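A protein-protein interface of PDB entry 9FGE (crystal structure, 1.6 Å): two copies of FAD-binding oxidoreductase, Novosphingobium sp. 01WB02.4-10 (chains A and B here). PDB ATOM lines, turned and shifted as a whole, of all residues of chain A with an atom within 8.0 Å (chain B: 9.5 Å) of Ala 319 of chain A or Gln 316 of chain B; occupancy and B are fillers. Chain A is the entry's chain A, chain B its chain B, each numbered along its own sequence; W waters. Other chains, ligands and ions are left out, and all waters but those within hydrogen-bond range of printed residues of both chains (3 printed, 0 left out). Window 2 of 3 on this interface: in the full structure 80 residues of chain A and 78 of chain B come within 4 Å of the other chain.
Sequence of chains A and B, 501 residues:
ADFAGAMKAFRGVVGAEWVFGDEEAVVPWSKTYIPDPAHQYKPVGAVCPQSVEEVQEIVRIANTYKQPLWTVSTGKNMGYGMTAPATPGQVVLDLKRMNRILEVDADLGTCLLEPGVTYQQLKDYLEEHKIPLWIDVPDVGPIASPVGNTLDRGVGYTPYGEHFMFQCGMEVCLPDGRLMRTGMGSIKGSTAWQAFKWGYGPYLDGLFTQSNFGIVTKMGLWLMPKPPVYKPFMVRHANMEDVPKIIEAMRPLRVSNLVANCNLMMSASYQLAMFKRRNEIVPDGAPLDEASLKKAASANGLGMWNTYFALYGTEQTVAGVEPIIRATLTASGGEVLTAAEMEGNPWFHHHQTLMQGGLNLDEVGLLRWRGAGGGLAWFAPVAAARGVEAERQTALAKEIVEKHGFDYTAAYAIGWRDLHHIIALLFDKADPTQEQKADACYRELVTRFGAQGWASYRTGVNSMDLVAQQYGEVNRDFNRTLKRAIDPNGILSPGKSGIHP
NE2 of Gln 316 of chain A lies within hydrogen-bond range of O of Ala 319 of chain B, 3.5 Å away.
The side-chain hydroxyl (OG1) of Thr 314 of chain A lies close to the backbone NH (N) of Gln 316 of chain A (3.2 Å). The backbone NH (N) of Thr 314 of chain A sits at hydrogen-bond distance from the side-chain hydroxyl (OG1) of Thr 317 of chain A, at 3.0 Å. The side-chain hydroxyl (OG1) of Thr 314 of chain B lies close to the backbone NH (N) of Gln 316 of chain B (3.2 Å). N of Thr 314 of chain B lies within hydrogen-bond range of OG1 of Thr 317 of chain B (2.9 Å).
NE2 of Gln 316 of chain A touches CA of Gly 320 of chain B, 3.9 Å away. Thr 317 of chain A touches Gly 320 of chain B (CG2 to O, 3.96 Å). Thr 317 of chain A touches Val 321 of chain B. Gln 316 of chain B touches Ala 319 of chain A. CA of Gly 320 of chain A touches NE2 of Gln 316 of chain B, at 3.9 Å. CG1 of Val 321 of chain A touches CG2 of Thr 317 of chain B (3.96 Å).
Printed residues of chain B within 4 Å of Gln 316 of chain A: Ala 319 and Gly 320. Printed residues of chain B within 4 Å of Thr 317 of chain A: Gly 320 and Val 321. Ala 319 of chain A touches one residue of chain B. Gly 320 of chain A touches just one residue of chain B: Gln 316. Of the printed residues of chain B, Val 321 of chain A touches Thr 317 (3.96 Å). Leu 311 of chain B touches none of the printed residues of chain A. Thr 314 of chain B touches none of the printed residues of chain A. Gln 316 of chain B touches two residues of chain A. Printed residues of chain A within 4 Å of Ala 319 of chain B: Gln 316. The nearest residue of chain A that does not touch Gln 316 of chain B is Gln 316 of chain A (4.9 Å). The nearest printed residue of chain A that does not touch Ala 319 of chain B is Thr 317 of chain A (6.7 Å).
Of the 14 printed residues of chain A, 5 touch a printed residue of chain B. Printed residues of chain A that touch a printed residue of chain B: Gln 316, Thr 317, Ala 319, Gly 320 and Val 321. Among the printed residues, 7 pairs touch across the chains.
Gln 316 of chain A touches Ala 319 of chain B, and with the chains exchanged Ala 319 of chain A touches Gln 316 of chain B. Gln 316 of chain A touches Gly 320 of chain B, and with the chains exchanged Gly 320 of chain A touches Gln 316 of chain B. Thr 317 of chain A touches Gly 320 of chain B, but with the chains exchanged Gly 320 of chain A does not touch Thr 317 of chain B (4.1 Å). Thr 317 of chain A touches Val 321 of chain B, and with the chains exchanged Val 321 of chain A touches Thr 317 of chain B. Positions printed for both chains: 229, 311, 314, 315, 316, 317, 318, 319, 320, 321, 322 and 323. Of the 7 pairs that touch across the chains among the printed residues, 6 have their exchanged pair printed and touching as well.
Water W1 lies within hydrogen-bond range of the side-chain amide nitrogen (NE2) of Gln 316 of chain A (2.6 Å), the backbone carbonyl oxygen (O) of Gln 316 of chain B (2.8 Å) and the backbone NH (N) of Gly 320 of chain B (3.5 Å). Water W2 bridges O of Gln 316 of chain A and NE2 of Gln 316 of chain B. Water W3 lies within hydrogen-bond range of O of Gly 320 of chain A (2.7 Å) and OG1 of Thr 314 of chain B (2.8 Å).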
ATOM      1  N   VAL A 229       3.492  15.092  -2.435  1.00  0.00           N
ATOM      2  CA  VAL A 229       2.514  14.098  -2.837  1.00  0.00           C
ATOM      3  C   VAL A 229       2.613  13.785  -4.343  1.00  0.00           C
ATOM      4  O   VAL A 229       2.619  14.690  -5.175  1.00  0.00           O
ATOM      5  CB  VAL A 229       1.101  14.560  -2.450  1.00  0.00           C
ATOM      6  CG1 VAL A 229       0.034  13.611  -2.933  1.00  0.00           C
ATOM      7  CG2 VAL A 229       1.041  14.745  -0.936  1.00  0.00           C
ATOM      8  N   LYS A 231       0.407  11.169  -6.908  1.00  0.00           N
ATOM      9  CA  LYS A 231      -0.808  10.375  -7.015  1.00  0.00           C
ATOM     10  C   LYS A 231      -1.028   9.902  -8.444  1.00  0.00           C
ATOM     11  O   LYS A 231      -1.411  10.697  -9.285  1.00  0.00           O
ATOM     12  CB  LYS A 231      -2.025  11.146  -6.553  1.00  0.00           C
ATOM     13  CG  LYS A 231      -3.260  10.265  -6.494  1.00  0.00           C
ATOM     14  CD  LYS A 231      -4.445  10.915  -5.812  1.00  0.00           C
ATOM     15  CE  LYS A 231      -5.564   9.932  -5.519  1.00  0.00           C
ATOM     16  NZ  LYS A 231      -6.678  10.631  -4.834  1.00  0.00           N
ATOM     17  N   LEU A 311      -0.970  13.239 -10.662  1.00  0.00           N
ATOM     18  CA  LEU A 311      -1.024  14.548 -10.004  1.00  0.00           C
ATOM     19  C   LEU A 311       0.129  14.654  -9.010  1.00  0.00           C
ATOM     20  O   LEU A 311       0.550  13.678  -8.375  1.00  0.00           O
ATOM     21  CB  LEU A 311      -2.415  14.715  -9.338  1.00  0.00           C
ATOM     22  CG  LEU A 311      -3.560  14.859 -10.327  1.00  0.00           C
ATOM     23  CD1 LEU A 311      -4.900  14.940  -9.599  1.00  0.00           C
ATOM     24  CD2 LEU A 311      -3.370  16.027 -11.280  1.00  0.00           C
ATOM     25  N   THR A 314       0.651  18.826  -3.299  1.00  0.00           N
ATOM     26  CA  THR A 314       0.225  18.475  -1.948  1.00  0.00           C
ATOM     27  C   THR A 314      -1.162  17.861  -1.979  1.00  0.00           C
ATOM     28  O   THR A 314      -1.842  17.938  -2.999  1.00  0.00           O
ATOM     29  CB  THR A 314       0.174  19.688  -1.021  1.00  0.00           C
ATOM     30  OG1 THR A 314      -0.861  20.568  -1.493  1.00  0.00           O
ATOM     31  CG2 THR A 314       1.528  20.359  -0.944  1.00  0.00           C
ATOM     32  N   GLU A 315      -1.590  17.327  -0.824  1.00  0.00           N
ATOM     33  CA  GLU A 315      -2.941  16.797  -0.716  1.00  0.00           C
ATOM     34  C   GLU A 315      -3.909  17.900  -1.151  1.00  0.00           C
ATOM     35  O   GLU A 315      -4.904  17.639  -1.810  1.00  0.00           O
ATOM     36  CB  GLU A 315      -3.236  16.285   0.703  1.00  0.00           C
ATOM     37  CG  GLU A 315      -2.303  15.176   1.189  1.00  0.00           C
ATOM     38  CD  GLU A 315      -0.979  15.598   1.842  1.00  0.00           C
ATOM     39  OE1 GLU A 315      -0.447  16.712   1.529  1.00  0.00           O
ATOM     40  OE2 GLU A 315      -0.461  14.811   2.695  1.00  0.00           O
ATOM     41  N   GLN A 316      -3.599  19.154  -0.823  1.00  0.00           N
ATOM     42  CA  GLN A 316      -4.537  20.222  -1.118  1.00  0.00           C
ATOM     43  C   GLN A 316      -4.531  20.589  -2.610  1.00  0.00           C
ATOM     44  O   GLN A 316      -5.590  20.770  -3.184  1.00  0.00           O
ATOM     45  CB  GLN A 316      -4.292  21.409  -0.189  1.00  0.00           C
ATOM     46  CG  GLN A 316      -5.584  22.138   0.107  1.00  0.00           C
ATOM     47  CD  GLN A 316      -5.407  23.231   1.128  1.00  0.00           C
ATOM     48  OE1 GLN A 316      -4.737  23.051   2.144  1.00  0.00           O
ATOM     49  NE2 GLN A 316      -6.005  24.379   0.849  1.00  0.00           N
ATOM     50  N   THR A 317      -3.361  20.701  -3.260  1.00  0.00           N
ATOM     51  CA  THR A 317      -3.333  21.041  -4.676  1.00  0.00           C
ATOM     52  C   THR A 317      -3.934  19.893  -5.493  1.00  0.00           C
ATOM     53  O   THR A 317      -4.690  20.152  -6.443  1.00  0.00           O
ATOM     54  CB  THR A 317      -1.927  21.424  -5.190  1.00  0.00           C
ATOM     55  OG1 THR A 317      -1.056  20.301  -5.222  1.00  0.00           O
ATOM     56  CG2 THR A 317      -1.287  22.484  -4.323  1.00  0.00           C
ATOM     57  N   VAL A 318      -3.655  18.642  -5.086  1.00  0.00           N
ATOM     58  CA  VAL A 318      -4.227  17.466  -5.740  1.00  0.00           C
ATOM     59  C   VAL A 318      -5.762  17.519  -5.655  1.00  0.00           C
ATOM     60  O   VAL A 318      -6.439  17.372  -6.667  1.00  0.00           O
ATOM     61  CB  VAL A 318      -3.651  16.155  -5.175  1.00  0.00           C
ATOM     62  CG1 VAL A 318      -4.457  14.948  -5.606  1.00  0.00           C
ATOM     63  CG2 VAL A 318      -2.181  15.985  -5.529  1.00  0.00           C
ATOM     64  N   ALA A 319      -6.304  17.838  -4.466  1.00  0.00           N
ATOM     65  CA  ALA A 319      -7.745  17.920  -4.274  1.00  0.00           C
ATOM     66  C   ALA A 319      -8.386  19.067  -5.049  1.00  0.00           C
ATOM     67  O   ALA A 319      -9.576  18.977  -5.341  1.00  0.00           O
ATOM     68  CB  ALA A 319      -8.087  18.003  -2.796  1.00  0.00           C
ATOM     69  N   GLY A 320      -7.623  20.125  -5.404  1.00  0.00           N
ATOM     70  CA  GLY A 320      -8.132  21.224  -6.215  1.00  0.00           C
ATOM     71  C   GLY A 320      -8.508  20.832  -7.646  1.00  0.00           C
ATOM     72  O   GLY A 320      -9.361  21.468  -8.286  1.00  0.00           O
ATOM     73  N   VAL A 321      -7.830  19.809  -8.195  1.00  0.00           N
ATOM     74  CA  VAL A 321      -8.057  19.496  -9.597  1.00  0.00           C
ATOM     75  C   VAL A 321      -8.665  18.111  -9.803  1.00  0.00           C
ATOM     76  O   VAL A 321      -9.295  17.886 -10.848  1.00  0.00           O
ATOM     77  CB  VAL A 321      -6.767  19.674 -10.411  1.00  0.00           C
ATOM     78  CG1 VAL A 321      -6.353  21.137 -10.437  1.00  0.00           C
ATOM     79  CG2 VAL A 321      -5.639  18.791  -9.919  1.00  0.00           C
ATOM     80  N   GLU A 322      -8.529  17.214  -8.831  1.00  0.00           N
ATOM     81  CA  GLU A 322      -8.925  15.818  -9.036  1.00  0.00           C
ATOM     82  C   GLU A 322     -10.415  15.714  -9.359  1.00  0.00           C
ATOM     83  O   GLU A 322     -10.803  14.988 -10.272  1.00  0.00           O
ATOM     84  CB  GLU A 322      -8.482  14.903  -7.894  1.00  0.00           C
ATOM     85  CG  GLU A 322      -8.965  13.489  -8.047  1.00  0.00           C
ATOM     86  CD  GLU A 322      -8.524  12.511  -6.983  1.00  0.00           C
ATOM     87  OE1 GLU A 322      -7.621  12.848  -6.191  1.00  0.00           O
ATOM     88  OE2 GLU A 322      -9.091  11.388  -6.970  1.00  0.00           O
ATOM     89  N   PRO A 323     -11.322  16.426  -8.670  1.00  0.00           N
ATOM     90  CA  PRO A 323     -12.726  16.344  -9.050  1.00  0.00           C
ATOM     91  C   PRO A 323     -13.064  16.711 -10.487  1.00  0.00           C
ATOM     92  O   PRO A 323     -13.869  16.007 -11.083  1.00  0.00           O
ATOM     93  CB  PRO A 323     -13.423  17.329  -8.081  1.00  0.00           C
ATOM     94  CG  PRO A 323     -12.494  17.337  -6.871  1.00  0.00           C
ATOM     95  CD  PRO A 323     -11.088  17.250  -7.459  1.00  0.00           C
ATOM     96  N   ILE A 324     -12.488  17.810 -11.026  1.00  0.00           N
ATOM     97  CA  ILE A 324     -12.789  18.232 -12.385  1.00  0.00           C
ATOM     98  C   ILE A 324     -12.258  17.188 -13.365  1.00  0.00           C
ATOM     99  O   ILE A 324     -12.867  16.914 -14.380  1.00  0.00           O
ATOM    100  CB  ILE A 324     -12.191  19.615 -12.722  1.00  0.00           C
ATOM    101  CG1 ILE A 324     -12.720  20.707 -11.793  1.00  0.00           C
ATOM    102  CG2 ILE A 324     -12.449  19.960 -14.178  1.00  0.00           C
ATOM    103  CD1 ILE A 324     -11.913  21.995 -11.820  1.00  0.00           C
ATOM    104  N   PRO B 228     -10.610  30.655 -14.378  1.00  0.00           N
ATOM    105  CA  PRO B 228     -11.791  31.101 -13.623  1.00  0.00           C
ATOM    106  C   PRO B 228     -11.452  32.186 -12.608  1.00  0.00           C
ATOM    107  O   PRO B 228     -12.200  33.167 -12.490  1.00  0.00           O
ATOM    108  CB  PRO B 228     -12.275  29.804 -12.954  1.00  0.00           C
ATOM    109  CG  PRO B 228     -11.740  28.669 -13.823  1.00  0.00           C
ATOM    110  CD  PRO B 228     -10.453  29.197 -14.438  1.00  0.00           C
ATOM    111  N   VAL B 229     -10.298  32.042 -11.965  1.00  0.00           N
ATOM    112  CA  VAL B 229      -9.819  32.995 -10.972  1.00  0.00           C
ATOM    113  C   VAL B 229      -8.381  33.448 -11.272  1.00  0.00           C
ATOM    114  O   VAL B 229      -7.475  32.637 -11.508  1.00  0.00           O
ATOM    115  CB  VAL B 229      -9.949  32.433  -9.546  1.00  0.00           C
ATOM    116  CG1 VAL B 229      -9.390  33.379  -8.480  1.00  0.00           C
ATOM    117  CG2 VAL B 229     -11.429  32.079  -9.322  1.00  0.00           C
ATOM    118  N   LEU B 311      -1.549  34.403  -8.945  1.00  0.00           N
ATOM    119  CA  LEU B 311      -2.043  33.027  -8.952  1.00  0.00           C
ATOM    120  C   LEU B 311      -3.242  32.921  -9.883  1.00  0.00           C
ATOM    121  O   LEU B 311      -4.041  33.875 -10.030  1.00  0.00           O
ATOM    122  CB  LEU B 311      -2.387  32.606  -7.507  1.00  0.00           C
ATOM    123  CG  LEU B 311      -1.184  32.500  -6.583  1.00  0.00           C
ATOM    124  CD1 LEU B 311      -1.588  32.157  -5.145  1.00  0.00           C
ATOM    125  CD2 LEU B 311      -0.157  31.528  -7.082  1.00  0.00           C
ATOM    126  N   TYR B 312      -3.318  31.745 -10.549  1.00  0.00           N
ATOM    127  CA  TYR B 312      -4.274  31.515 -11.606  1.00  0.00           C
ATOM    128  C   TYR B 312      -4.906  30.132 -11.412  1.00  0.00           C
ATOM    129  O   TYR B 312      -4.173  29.181 -11.150  1.00  0.00           O
ATOM    130  CB  TYR B 312      -3.613  31.547 -12.992  1.00  0.00           C
ATOM    131  CG  TYR B 312      -2.710  32.735 -13.239  1.00  0.00           C
ATOM    132  CD1 TYR B 312      -1.410  32.719 -12.783  1.00  0.00           C
ATOM    133  CD2 TYR B 312      -3.147  33.855 -13.917  1.00  0.00           C
ATOM    134  CE1 TYR B 312      -0.581  33.805 -13.004  1.00  0.00           C
ATOM    135  CE2 TYR B 312      -2.323  34.945 -14.150  1.00  0.00           C
ATOM    136  CZ  TYR B 312      -1.025  34.908 -13.707  1.00  0.00           C
ATOM    137  OH  TYR B 312      -0.158  35.956 -13.954  1.00  0.00           O
ATOM    138  N   GLY B 313      -6.229  30.076 -11.508  1.00  0.00           N
ATOM    139  CA  GLY B 313      -6.960  28.812 -11.394  1.00  0.00           C
ATOM    140  C   GLY B 313      -8.391  28.972 -10.875  1.00  0.00           C
ATOM    141  O   GLY B 313      -9.212  29.720 -11.395  1.00  0.00           O
ATOM    142  N   THR B 314      -8.675  28.247  -9.793  1.00  0.00           N
ATOM    143  CA  THR B 314      -9.913  28.393  -9.056  1.00  0.00           C
ATOM    144  C   THR B 314      -9.608  28.872  -7.652  1.00  0.00           C
ATOM    145  O   THR B 314      -8.448  28.868  -7.226  1.00  0.00           O
ATOM    146  CB  THR B 314     -10.642  27.047  -8.949  1.00  0.00           C
ATOM    147  OG1 THR B 314      -9.823  26.167  -8.166  1.00  0.00           O
ATOM    148  CG2 THR B 314     -10.933  26.442 -10.309  1.00  0.00           C
ATOM    149  N   GLU B 315     -10.676  29.161  -6.912  1.00  0.00           N
ATOM    150  CA  GLU B 315     -10.532  29.609  -5.541  1.00  0.00           C
ATOM    151  C   GLU B 315      -9.790  28.514  -4.768  1.00  0.00           C
ATOM    152  O   GLU B 315      -8.936  28.788  -3.930  1.00  0.00           O
ATOM    153  CB  GLU B 315     -11.916  29.979  -4.994  1.00  0.00           C
ATOM    154  CG  GLU B 315     -12.621  31.074  -5.800  1.00  0.00           C
ATOM    155  CD  GLU B 315     -13.477  30.693  -7.019  1.00  0.00           C
ATOM    156  OE1 GLU B 315     -13.302  29.578  -7.631  1.00  0.00           O
ATOM    157  OE2 GLU B 315     -14.366  31.525  -7.379  1.00  0.00           O
ATOM    158  N   GLN B 316     -10.037  27.248  -5.133  1.00  0.00           N
ATOM    159  CA  GLN B 316      -9.452  26.137  -4.400  1.00  0.00           C
ATOM    160  C   GLN B 316      -7.981  25.903  -4.772  1.00  0.00           C
ATOM    161  O   GLN B 316      -7.174  25.659  -3.871  1.00  0.00           O
ATOM    162  CB  GLN B 316     -10.310  24.870  -4.515  1.00  0.00           C
ATOM    163  CG  GLN B 316     -10.149  23.987  -3.284  1.00  0.00           C
ATOM    164  CD  GLN B 316     -11.026  22.757  -3.310  1.00  0.00           C
ATOM    165  OE1 GLN B 316     -12.239  22.844  -3.491  1.00  0.00           O
ATOM    166  NE2 GLN B 316     -10.421  21.597  -3.121  1.00  0.00           N
ATOM    167  N   THR B 317      -7.606  25.984  -6.064  1.00  0.00           N
ATOM    168  CA  THR B 317      -6.199  25.845  -6.439  1.00  0.00           C
ATOM    169  C   THR B 317      -5.377  26.999  -5.861  1.00  0.00           C
ATOM    170  O   THR B 317      -4.265  26.770  -5.380  1.00  0.00           O
ATOM    171  CB  THR B 317      -5.977  25.722  -7.961  1.00  0.00           C
ATOM    172  OG1 THR B 317      -6.325  26.956  -8.573  1.00  0.00           O
ATOM    173  CG2 THR B 317      -6.784  24.595  -8.563  1.00  0.00           C
ATOM    174  N   VAL B 318      -5.923  28.219  -5.840  1.00  0.00           N
ATOM    175  CA  VAL B 318      -5.218  29.365  -5.268  1.00  0.00           C
ATOM    176  C   VAL B 318      -4.974  29.122  -3.769  1.00  0.00           C
ATOM    177  O   VAL B 318      -3.847  29.270  -3.302  1.00  0.00           O
ATOM    178  CB  VAL B 318      -5.983  30.668  -5.536  1.00  0.00           C
ATOM    179  CG1 VAL B 318      -5.439  31.855  -4.747  1.00  0.00           C
ATOM    180  CG2 VAL B 318      -6.028  30.968  -7.038  1.00  0.00           C
ATOM    181  N   ALA B 319      -6.019  28.694  -3.031  1.00  0.00           N
ATOM    182  CA  ALA B 319      -5.907  28.393  -1.605  1.00  0.00           C
ATOM    183  C   ALA B 319      -4.900  27.278  -1.300  1.00  0.00           C
ATOM    184  O   ALA B 319      -4.350  27.237  -0.202  1.00  0.00           O
ATOM    185  CB  ALA B 319      -7.262  28.059  -1.039  1.00  0.00           C
ATOM    186  N   GLY B 320      -4.648  26.375  -2.262  1.00  0.00           N
ATOM    187  CA  GLY B 320      -3.652  25.333  -2.112  1.00  0.00           C
ATOM    188  C   GLY B 320      -2.219  25.849  -1.965  1.00  0.00           C
ATOM    189  O   GLY B 320      -1.386  25.152  -1.394  1.00  0.00           O
ATOM    190  N   VAL B 321      -1.896  27.041  -2.510  1.00  0.00           N
ATOM    191  CA  VAL B 321      -0.504  27.457  -2.541  1.00  0.00           C
ATOM    192  C   VAL B 321      -0.281  28.789  -1.815  1.00  0.00           C
ATOM    193  O   VAL B 321       0.838  29.052  -1.363  1.00  0.00           O
ATOM    194  CB  VAL B 321       0.036  27.466  -3.980  1.00  0.00           C
ATOM    195  CG1 VAL B 321       0.101  26.058  -4.552  1.00  0.00           C
ATOM    196  CG2 VAL B 321      -0.747  28.392  -4.881  1.00  0.00           C
ATOM    197  N   GLU B 322      -1.330  29.581  -1.640  1.00  0.00           N
ATOM    198  CA  GLU B 322      -1.186  30.932  -1.129  1.00  0.00           C
ATOM    199  C   GLU B 322      -0.590  30.903   0.272  1.00  0.00           C
ATOM    200  O   GLU B 322       0.263  31.729   0.579  1.00  0.00           O
ATOM    201  CB  GLU B 322      -2.505  31.683  -1.147  1.00  0.00           C
ATOM    202  CG  GLU B 322      -2.424  33.084  -0.603  1.00  0.00           C
ATOM    203  CD  GLU B 322      -3.688  33.906  -0.733  1.00  0.00           C
ATOM    204  OE1 GLU B 322      -4.576  33.573  -1.541  1.00  0.00           O
ATOM    205  OE2 GLU B 322      -3.764  34.940  -0.028  1.00  0.00           O
ATOM    206  N   PRO B 323      -1.019  30.013   1.197  1.00  0.00           N
ATOM    207  CA  PRO B 323      -0.400  30.014   2.525  1.00  0.00           C
ATOM    208  C   PRO B 323       1.110  29.788   2.547  1.00  0.00           C
ATOM    209  O   PRO B 323       1.819  30.457   3.306  1.00  0.00           O
ATOM    210  CB  PRO B 323      -1.148  28.867   3.257  1.00  0.00           C
ATOM    211  CG  PRO B 323      -2.498  28.821   2.554  1.00  0.00           C
ATOM    212  CD  PRO B 323      -2.154  29.063   1.086  1.00  0.00           C
HETATM  213  O   HOH W   1      -7.359  24.423  -1.342  1.00  0.00           O
HETATM  214  O   HOH W   2      -7.847  21.577  -2.072  1.00  0.00           O
HETATM  215  O   HOH W   3     -10.922  23.653  -7.787  1.00  0.00           O
